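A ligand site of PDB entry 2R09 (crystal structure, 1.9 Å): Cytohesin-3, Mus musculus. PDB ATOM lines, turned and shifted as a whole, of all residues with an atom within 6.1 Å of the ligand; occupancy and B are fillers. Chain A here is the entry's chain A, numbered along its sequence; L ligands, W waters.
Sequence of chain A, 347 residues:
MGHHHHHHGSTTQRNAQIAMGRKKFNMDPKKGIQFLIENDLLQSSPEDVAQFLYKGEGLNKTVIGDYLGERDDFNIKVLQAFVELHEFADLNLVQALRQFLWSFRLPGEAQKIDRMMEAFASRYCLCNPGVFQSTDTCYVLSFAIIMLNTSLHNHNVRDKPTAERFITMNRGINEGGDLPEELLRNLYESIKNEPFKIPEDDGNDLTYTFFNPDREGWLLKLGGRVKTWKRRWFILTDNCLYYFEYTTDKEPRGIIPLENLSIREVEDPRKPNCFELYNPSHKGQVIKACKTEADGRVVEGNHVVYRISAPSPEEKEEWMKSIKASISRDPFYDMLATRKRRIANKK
The guanidinium group of Arg 253 lies within salt-bridge range of an oxygen (O11) of the ligand (3.0 Å).
O13 of the ligand is in salt-bridge range of NZ of Lys 221, at 2.9 Å.
The backbone NH (N) of Arg 225 is in hydrogen-bond range of an oxygen (O17) of the ligand, at 2.8 Å.
An oxygen (O17) of the ligand is in hydrogen-bond range of the side-chain amide nitrogen of Asn 302, 3.0 Å away.
An oxygen (O18) of the ligand lies within hydrogen-bond range of the backbone NH (N) of Val 226 (3.1 Å).
O8 of the ligand is in salt-bridge range of NZ of Lys 230, at 3.6 Å.
The side-chain hydroxyl (OH) of Tyr 243 lies within hydrogen-bond range of an oxygen (O15) of the ligand (2.5 Å).
A ring nitrogen (NE2) of His 303 lies within hydrogen-bond range of an oxygen (O13) of the ligand (2.7 Å).
NZ of Lys 291 is in salt-bridge range of O16 of the ligand, at 2.7 Å.
The side-chain hydroxyl of Thr 228 lies within hydrogen-bond range of an oxygen (O7) of the ligand, at 2.8 Å.
An oxygen (O5) of the ligand is in hydrogen-bond range of the backbone NH (N) of Gly 224.
The guanidinium group (NE) of Arg 232 lies within salt-bridge range of an oxygen (O12) of the ligand (2.8 Å).
N of Tyr 243 sits at hydrogen-bond distance from O of Gly 254 (3.1 Å).
N of Arg 253 lies within hydrogen-bond range of O of Tyr 243 (2.7 Å).
The backbone NH (N) of Lys 230 sits at hydrogen-bond distance from the backbone carbonyl oxygen (O) of Lys 221, 2.8 Å away.
N of Gly 223 is in hydrogen-bond range of O of Thr 228.
A ring nitrogen (NE2) of His 303 lies within hydrogen-bond range of the backbone NH (N) of Gly 224 (3.3 Å).
The backbone carbonyl oxygen (O) of Gly 223 sits at hydrogen-bond distance from the side-chain amino group (NZ) of Lys 227, at 3.2 Å.
The backbone carbonyl oxygen (O) of Arg 253 sits at hydrogen-bond distance from the backbone NH (N) of Thr 292, 2.9 Å away.
The side-chain amino group (NZ) of Lys 227 sits at hydrogen-bond distance from the backbone carbonyl oxygen (O) of Gly 224 (2.9 Å).
Merely in contact with the ligand: Gly 223.
Hydrophobic or aromatic side chains within 4 Å of the ligand: Val 226, Tyr 243 and His 303.
Within 4 Å of the ligand: Lys 221, Gly 223, Gly 224, Arg 225, Val 226, Thr 228, Lys 230, Arg 232, Tyr 243, Arg 253, Lys 291, Asn 302 and His 303.
Water W10 lies within hydrogen-bond range of O14 of the ligand (2.6 Å), N of Asn 302 (2.8 Å) and NZ of Lys 291 (3.4 Å).
Water W8 bridges an oxygen (O18) of the ligand and the guanidinium group of Arg 225.
Water W1 lies within hydrogen-bond range of OE2 of Glu 293, O16 of the ligand and ND2 of Asn 302.
Water W7 bridges the side-chain carboxylate (OE1) of Glu 293 (2.7 Å) and an oxygen (O16) of the ligand (2.7 Å).
Water W11 lies within hydrogen-bond range of OH of Tyr 306 (2.6 Å), OH of Tyr 243 (2.7 Å) and O14 of the ligand (2.8 Å).
Water W6 lies within hydrogen-bond range of O10 of the ligand (2.8 Å), O of Thr 292 (2.8 Å) and NZ of Lys 291 (3.0 Å).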
ATOM      1  N   LYS A 221      -6.543   9.973 -28.072  1.00  0.00           N
ATOM      2  CA  LYS A 221      -5.271   9.838 -27.358  1.00  0.00           C
ATOM      3  C   LYS A 221      -5.477   9.699 -25.851  1.00  0.00           C
ATOM      4  O   LYS A 221      -6.364  10.330 -25.272  1.00  0.00           O
ATOM      5  CB  LYS A 221      -4.324  11.001 -27.688  1.00  0.00           C
ATOM      6  CG  LYS A 221      -4.837  12.403 -27.299  1.00  0.00           C
ATOM      7  CD  LYS A 221      -3.695  13.447 -27.310  1.00  0.00           C
ATOM      8  CE  LYS A 221      -2.920  13.419 -25.998  1.00  0.00           C
ATOM      9  NZ  LYS A 221      -3.772  13.856 -24.846  1.00  0.00           N
ATOM     10  N   LEU A 222      -4.645   8.861 -25.242  1.00  0.00           N
ATOM     11  CA  LEU A 222      -4.677   8.644 -23.791  1.00  0.00           C
ATOM     12  C   LEU A 222      -3.818   9.694 -23.075  1.00  0.00           C
ATOM     13  O   LEU A 222      -2.743  10.031 -23.555  1.00  0.00           O
ATOM     14  CB  LEU A 222      -4.175   7.236 -23.468  1.00  0.00           C
ATOM     15  CG  LEU A 222      -4.120   6.795 -22.005  1.00  0.00           C
ATOM     16  CD1 LEU A 222      -5.484   6.899 -21.376  1.00  0.00           C
ATOM     17  CD2 LEU A 222      -3.582   5.362 -21.894  1.00  0.00           C
ATOM     18  N   GLY A 223      -4.308  10.191 -21.937  1.00  0.00           N
ATOM     19  CA  GLY A 223      -3.599  11.225 -21.157  1.00  0.00           C
ATOM     20  C   GLY A 223      -2.371  10.730 -20.394  1.00  0.00           C
ATOM     21  O   GLY A 223      -2.063   9.549 -20.411  1.00  0.00           O
ATOM     22  N   GLY A 224      -1.685  11.661 -19.721  1.00  0.00           N
ATOM     23  CA  GLY A 224      -0.404  11.358 -19.040  1.00  0.00           C
ATOM     24  C   GLY A 224      -0.630  10.907 -17.616  1.00  0.00           C
ATOM     25  O   GLY A 224      -0.837   9.718 -17.365  1.00  0.00           O
ATOM     26  N   ARG A 225      -0.615  11.851 -16.675  1.00  0.00           N
ATOM     27  CA  ARG A 225      -0.891  11.543 -15.275  1.00  0.00           C
ATOM     28  C   ARG A 225      -2.311  11.055 -15.106  1.00  0.00           C
ATOM     29  O   ARG A 225      -2.566  10.046 -14.455  1.00  0.00           O
ATOM     30  CB  ARG A 225      -0.651  12.753 -14.371  1.00  0.00           C
ATOM     31  CG  ARG A 225       0.783  13.289 -14.368  1.00  0.00           C
ATOM     32  CD  ARG A 225       0.921  14.551 -13.524  1.00  0.00           C
ATOM     33  NE  ARG A 225       0.778  14.304 -12.093  1.00  0.00           N
ATOM     34  CZ  ARG A 225      -0.338  14.541 -11.395  1.00  0.00           C
ATOM     35  NH1 ARG A 225      -1.398  15.092 -11.979  1.00  0.00           N
ATOM     36  NH2 ARG A 225      -0.366  14.291 -10.096  1.00  0.00           N
ATOM     37  N   VAL A 226      -3.251  11.773 -15.699  1.00  0.00           N
ATOM     38  CA  VAL A 226      -4.654  11.403 -15.638  1.00  0.00           C
ATOM     39  C   VAL A 226      -4.992  10.651 -16.915  1.00  0.00           C
ATOM     40  O   VAL A 226      -4.903  11.209 -18.016  1.00  0.00           O
ATOM     41  CB  VAL A 226      -5.567  12.635 -15.465  1.00  0.00           C
ATOM     42  CG1 VAL A 226      -7.046  12.232 -15.486  1.00  0.00           C
ATOM     43  CG2 VAL A 226      -5.233  13.379 -14.167  1.00  0.00           C
ATOM     44  N   LYS A 227      -5.419   9.401 -16.748  1.00  0.00           N
ATOM     45  CA  LYS A 227      -5.595   8.442 -17.841  1.00  0.00           C
ATOM     46  C   LYS A 227      -6.934   8.550 -18.564  1.00  0.00           C
ATOM     47  O   LYS A 227      -7.704   7.596 -18.615  1.00  0.00           O
ATOM     48  CB  LYS A 227      -5.363   7.006 -17.322  1.00  0.00           C
ATOM     49  CG  LYS A 227      -3.950   6.768 -16.818  1.00  0.00           C
ATOM     50  CD  LYS A 227      -2.979   6.969 -17.966  1.00  0.00           C
ATOM     51  CE  LYS A 227      -1.553   6.736 -17.578  1.00  0.00           C
ATOM     52  NZ  LYS A 227      -0.710   7.182 -18.713  1.00  0.00           N
ATOM     53  N   THR A 228      -7.193   9.726 -19.124  1.00  0.00           N
ATOM     54  CA  THR A 228      -8.420   9.939 -19.886  1.00  0.00           C
ATOM     55  C   THR A 228      -8.161   9.967 -21.396  1.00  0.00           C
ATOM     56  O   THR A 228      -7.096  10.397 -21.866  1.00  0.00           O
ATOM     57  CB  THR A 228      -9.180  11.200 -19.422  1.00  0.00           C
ATOM     58  OG1 THR A 228      -8.305  12.327 -19.459  1.00  0.00           O
ATOM     59  CG2 THR A 228      -9.685  11.008 -17.988  1.00  0.00           C
ATOM     60  N   TRP A 229      -9.147   9.494 -22.153  1.00  0.00           N
ATOM     61  CA  TRP A 229      -9.055   9.467 -23.611  1.00  0.00           C
ATOM     62  C   TRP A 229      -9.729  10.706 -24.195  1.00  0.00           C
ATOM     63  O   TRP A 229     -10.889  11.009 -23.871  1.00  0.00           O
ATOM     64  CB  TRP A 229      -9.708   8.201 -24.165  1.00  0.00           C
ATOM     65  CG  TRP A 229      -8.941   6.931 -23.881  1.00  0.00           C
ATOM     66  CD1 TRP A 229      -9.097   6.111 -22.791  1.00  0.00           C
ATOM     67  CD2 TRP A 229      -7.947   6.326 -24.700  1.00  0.00           C
ATOM     68  NE1 TRP A 229      -8.246   5.032 -22.889  1.00  0.00           N
ATOM     69  CE2 TRP A 229      -7.525   5.141 -24.056  1.00  0.00           C
ATOM     70  CE3 TRP A 229      -7.361   6.674 -25.927  1.00  0.00           C
ATOM     71  CZ2 TRP A 229      -6.543   4.302 -24.592  1.00  0.00           C
ATOM     72  CZ3 TRP A 229      -6.383   5.844 -26.459  1.00  0.00           C
ATOM     73  CH2 TRP A 229      -5.982   4.665 -25.789  1.00  0.00           C
ATOM     74  N   LYS A 230      -8.989  11.410 -25.049  1.00  0.00           N
ATOM     75  CA  LYS A 230      -9.465  12.644 -25.671  1.00  0.00           C
ATOM     76  C   LYS A 230      -9.382  12.596 -27.183  1.00  0.00           C
ATOM     77  O   LYS A 230      -8.364  12.164 -27.747  1.00  0.00           O
ATOM     78  CB  LYS A 230      -8.655  13.846 -25.167  1.00  0.00           C
ATOM     79  CG  LYS A 230      -8.791  14.115 -23.675  1.00  0.00           C
ATOM     80  CD  LYS A 230     -10.239  14.448 -23.307  1.00  0.00           C
ATOM     81  CE  LYS A 230     -10.449  14.364 -21.799  1.00  0.00           C
ATOM     82  NZ  LYS A 230     -11.773  14.937 -21.408  1.00  0.00           N
ATOM     83  N   ARG A 232      -8.627  14.253 -30.510  1.00  0.00           N
ATOM     84  CA  ARG A 232      -7.747  15.360 -30.865  1.00  0.00           C
ATOM     85  C   ARG A 232      -7.398  15.328 -32.344  1.00  0.00           C
ATOM     86  O   ARG A 232      -7.377  14.267 -32.981  1.00  0.00           O
ATOM     87  CB  ARG A 232      -6.466  15.346 -30.006  1.00  0.00           C
ATOM     88  CG  ARG A 232      -6.697  15.565 -28.490  1.00  0.00           C
ATOM     89  CD  ARG A 232      -7.123  16.999 -28.158  1.00  0.00           C
ATOM     90  NE  ARG A 232      -7.413  17.195 -26.726  1.00  0.00           N
ATOM     91  CZ  ARG A 232      -8.645  17.334 -26.216  1.00  0.00           C
ATOM     92  NH1 ARG A 232      -9.713  17.299 -27.010  1.00  0.00           N
ATOM     93  NH2 ARG A 232      -8.813  17.518 -24.910  1.00  0.00           N
ATOM     94  N   TYR A 243      -0.953  18.220 -31.865  1.00  0.00           N
ATOM     95  CA  TYR A 243      -2.370  17.914 -31.694  1.00  0.00           C
ATOM     96  C   TYR A 243      -3.146  19.098 -31.146  1.00  0.00           C
ATOM     97  O   TYR A 243      -2.618  19.898 -30.375  1.00  0.00           O
ATOM     98  CB  TYR A 243      -2.577  16.621 -30.888  1.00  0.00           C
ATOM     99  CG  TYR A 243      -1.961  16.619 -29.511  1.00  0.00           C
ATOM    100  CD1 TYR A 243      -2.734  16.860 -28.383  1.00  0.00           C
ATOM    101  CD2 TYR A 243      -0.595  16.328 -29.329  1.00  0.00           C
ATOM    102  CE1 TYR A 243      -2.176  16.834 -27.091  1.00  0.00           C
ATOM    103  CE2 TYR A 243      -0.020  16.311 -28.039  1.00  0.00           C
ATOM    104  CZ  TYR A 243      -0.821  16.558 -26.935  1.00  0.00           C
ATOM    105  OH  TYR A 243      -0.283  16.542 -25.667  1.00  0.00           O
ATOM    106  N   ARG A 253      -2.779  21.920 -28.663  1.00  0.00           N
ATOM    107  CA  ARG A 253      -2.948  21.446 -27.309  1.00  0.00           C
ATOM    108  C   ARG A 253      -1.604  20.895 -26.845  1.00  0.00           C
ATOM    109  O   ARG A 253      -1.237  21.060 -25.681  1.00  0.00           O
ATOM    110  CB  ARG A 253      -4.036  20.375 -27.242  1.00  0.00           C
ATOM    111  CG  ARG A 253      -4.292  19.787 -25.856  1.00  0.00           C
ATOM    112  CD  ARG A 253      -4.680  20.832 -24.820  1.00  0.00           C
ATOM    113  NE  ARG A 253      -5.861  21.631 -25.195  1.00  0.00           N
ATOM    114  CZ  ARG A 253      -7.098  21.435 -24.745  1.00  0.00           C
ATOM    115  NH1 ARG A 253      -7.382  20.428 -23.909  1.00  0.00           N
ATOM    116  NH2 ARG A 253      -8.079  22.228 -25.148  1.00  0.00           N
ATOM    117  N   GLY A 254      -0.866  20.276 -27.772  1.00  0.00           N
ATOM    118  CA  GLY A 254       0.435  19.724 -27.444  1.00  0.00           C
ATOM    119  C   GLY A 254       1.331  19.548 -28.653  1.00  0.00           C
ATOM    120  O   GLY A 254       0.864  19.572 -29.800  1.00  0.00           O
ATOM    121  N   LYS A 291       2.742  20.925 -23.676  1.00  0.00           N
ATOM    122  CA  LYS A 291       1.301  21.024 -23.854  1.00  0.00           C
ATOM    123  C   LYS A 291       0.762  22.158 -23.006  1.00  0.00           C
ATOM    124  O   LYS A 291       1.464  22.700 -22.136  1.00  0.00           O
ATOM    125  CB  LYS A 291       0.617  19.696 -23.492  1.00  0.00           C
ATOM    126  CG  LYS A 291       1.049  19.090 -22.140  1.00  0.00           C
ATOM    127  CD  LYS A 291       0.400  19.795 -20.947  1.00  0.00           C
ATOM    128  CE  LYS A 291       0.248  18.834 -19.758  1.00  0.00           C
ATOM    129  NZ  LYS A 291      -0.789  17.805 -20.030  1.00  0.00           N
ATOM    130  N   THR A 292      -0.508  22.514 -23.231  1.00  0.00           N
ATOM    131  CA  THR A 292      -1.137  23.577 -22.468  1.00  0.00           C
ATOM    132  C   THR A 292      -2.091  23.029 -21.419  1.00  0.00           C
ATOM    133  O   THR A 292      -2.739  22.005 -21.627  1.00  0.00           O
ATOM    134  CB  THR A 292      -1.930  24.541 -23.376  1.00  0.00           C
ATOM    135  OG1 THR A 292      -2.996  23.813 -23.994  1.00  0.00           O
ATOM    136  CG2 THR A 292      -1.042  25.118 -24.467  1.00  0.00           C
ATOM    137  N   GLU A 293      -2.139  23.722 -20.289  1.00  0.00           N
ATOM    138  CA  GLU A 293      -3.070  23.420 -19.201  1.00  0.00           C
ATOM    139  C   GLU A 293      -4.302  24.296 -19.372  1.00  0.00           C
ATOM    140  O   GLU A 293      -4.271  25.272 -20.131  1.00  0.00           O
ATOM    141  CB  GLU A 293      -2.415  23.700 -17.845  1.00  0.00           C
ATOM    142  CG  GLU A 293      -1.182  22.871 -17.520  1.00  0.00           C
ATOM    143  CD  GLU A 293      -1.508  21.493 -16.951  1.00  0.00           C
ATOM    144  OE1 GLU A 293      -2.672  21.050 -17.023  1.00  0.00           O
ATOM    145  OE2 GLU A 293      -0.579  20.840 -16.447  1.00  0.00           O
ATOM    146  N   GLY A 301       5.236  17.809 -20.978  1.00  0.00           N
ATOM    147  CA  GLY A 301       4.399  16.612 -20.911  1.00  0.00           C
ATOM    148  C   GLY A 301       4.869  15.657 -19.819  1.00  0.00           C
ATOM    149  O   GLY A 301       6.041  15.708 -19.392  1.00  0.00           O
ATOM    150  N   ASN A 302       3.979  14.776 -19.400  1.00  0.00           N
ATOM    151  CA  ASN A 302       4.253  13.801 -18.338  1.00  0.00           C
ATOM    152  C   ASN A 302       4.218  12.362 -18.842  1.00  0.00           C
ATOM    153  O   ASN A 302       4.087  11.420 -18.042  1.00  0.00           O
ATOM    154  CB  ASN A 302       3.221  13.975 -17.212  1.00  0.00           C
ATOM    155  CG  ASN A 302       3.149  15.408 -16.693  1.00  0.00           C
ATOM    156  OD1 ASN A 302       4.161  15.999 -16.349  1.00  0.00           O
ATOM    157  ND2 ASN A 302       1.942  15.964 -16.615  1.00  0.00           N
ATOM    158  N   HIS A 303       4.305  12.180 -20.160  1.00  0.00           N
ATOM    159  CA  HIS A 303       4.153  10.856 -20.771  1.00  0.00           C
ATOM    160  C   HIS A 303       5.454  10.082 -20.849  1.00  0.00           C
ATOM    161  O   HIS A 303       6.449  10.603 -21.349  1.00  0.00           O
ATOM    162  CB  HIS A 303       3.632  10.972 -22.202  1.00  0.00           C
ATOM    163  CG  HIS A 303       2.198  11.358 -22.309  1.00  0.00           C
ATOM    164  ND1 HIS A 303       1.216  10.478 -22.703  1.00  0.00           N
ATOM    165  CD2 HIS A 303       1.574  12.542 -22.079  1.00  0.00           C
ATOM    166  CE1 HIS A 303       0.043  11.097 -22.715  1.00  0.00           C
ATOM    167  NE2 HIS A 303       0.239  12.365 -22.354  1.00  0.00           N
ATOM    168  N   TYR A 306       2.989   7.749 -25.475  1.00  0.00           N
ATOM    169  CA  TYR A 306       1.762   8.359 -26.009  1.00  0.00           C
ATOM    170  C   TYR A 306       0.985   7.267 -26.689  1.00  0.00           C
ATOM    171  O   TYR A 306       1.376   6.810 -27.765  1.00  0.00           O
ATOM    172  CB  TYR A 306       2.087   9.480 -27.022  1.00  0.00           C
ATOM    173  CG  TYR A 306       2.490  10.770 -26.341  1.00  0.00           C
ATOM    174  CD1 TYR A 306       1.524  11.692 -25.951  1.00  0.00           C
ATOM    175  CD2 TYR A 306       3.838  11.050 -26.092  1.00  0.00           C
ATOM    176  CE1 TYR A 306       1.898  12.890 -25.311  1.00  0.00           C
ATOM    177  CE2 TYR A 306       4.216  12.240 -25.454  1.00  0.00           C
ATOM    178  CZ  TYR A 306       3.236  13.144 -25.064  1.00  0.00           C
ATOM    179  OH  TYR A 306       3.586  14.320 -24.423  1.00  0.00           O
HETATM  180  C1  LIG L   1      -6.162  15.437 -19.252  1.00  0.00           C
HETATM  181  O1  LIG L   1      -7.299  14.837 -18.617  1.00  0.00           O
HETATM  182  C2  LIG L   1      -6.170  15.095 -20.743  1.00  0.00           C
HETATM  183  O2  LIG L   1      -6.121  13.672 -20.941  1.00  0.00           O
HETATM  184  C3  LIG L   1      -4.965  15.779 -21.410  1.00  0.00           C
HETATM  185  O3  LIG L   1      -5.036  15.636 -22.829  1.00  0.00           O
HETATM  186  C4  LIG L   1      -3.640  15.250 -20.854  1.00  0.00           C
HETATM  187  O4  LIG L   1      -2.568  16.019 -21.389  1.00  0.00           O
HETATM  188  C5  LIG L   1      -3.599  15.417 -19.329  1.00  0.00           C
HETATM  189  O5  LIG L   1      -2.430  14.708 -18.893  1.00  0.00           O
HETATM  190  C6  LIG L   1      -4.864  14.926 -18.602  1.00  0.00           C
HETATM  191  O6  LIG L   1      -4.848  15.312 -17.209  1.00  0.00           O
HETATM  192  P1  LIG L   1      -8.710  15.614 -18.439  1.00  0.00           P
HETATM  193  O7  LIG L   1      -9.609  14.441 -18.196  1.00  0.00           O
HETATM  194  O8  LIG L   1      -8.966  16.368 -19.723  1.00  0.00           O
HETATM  195  O9  LIG L   1      -8.510  16.510 -17.248  1.00  0.00           O
HETATM  196  P2  LIG L   1      -5.209  16.934 -23.763  1.00  0.00           P
HETATM  197  O10 LIG L   1      -3.953  17.748 -23.468  1.00  0.00           O
HETATM  198  O11 LIG L   1      -6.478  17.641 -23.318  1.00  0.00           O
HETATM  199  O12 LIG L   1      -5.243  16.374 -25.162  1.00  0.00           O
HETATM  200  P3  LIG L   1      -1.571  15.471 -22.523  1.00  0.00           P
HETATM  201  O13 LIG L   1      -1.858  13.997 -22.660  1.00  0.00           O
HETATM  202  O14 LIG L   1      -0.214  15.805 -21.974  1.00  0.00           O
HETATM  203  O15 LIG L   1      -1.929  16.266 -23.754  1.00  0.00           O
HETATM  204  P4  LIG L   1      -1.613  15.128 -17.582  1.00  0.00           P
HETATM  205  O16 LIG L   1      -1.426  16.628 -17.647  1.00  0.00           O
HETATM  206  O17 LIG L   1      -0.307  14.390 -17.739  1.00  0.00           O
HETATM  207  O18 LIG L   1      -2.461  14.645 -16.443  1.00  0.00           O
HETATM  208  O   HOH W   1       0.059  18.366 -16.174  1.00  0.00           O
HETATM  209  O   HOH W   2      -7.690  18.289 -20.934  1.00  0.00           O
HETATM  210  O   HOH W   3     -12.211  14.302 -18.723  1.00  0.00           O
HETATM  211  O   HOH W   4      -5.707  12.601 -23.575  1.00  0.00           O
HETATM  212  O   HOH W   5     -10.584  13.755 -15.600  1.00  0.00           O
HETATM  213  O   HOH W   6      -3.136  19.255 -21.301  1.00  0.00           O
HETATM  214  O   HOH W   7      -3.337  18.471 -17.029  1.00  0.00           O
HETATM  215  O   HOH W   8      -2.140  16.330 -14.396  1.00  0.00           O
HETATM  216  O   HOH W   9      -7.766  19.192 -17.869  1.00  0.00           O
HETATM  217  O   HOH W  10       1.198  15.000 -19.891  1.00  0.00           O
HETATM  218  O   HOH W  11       1.734  16.050 -23.913  1.00  0.00           O
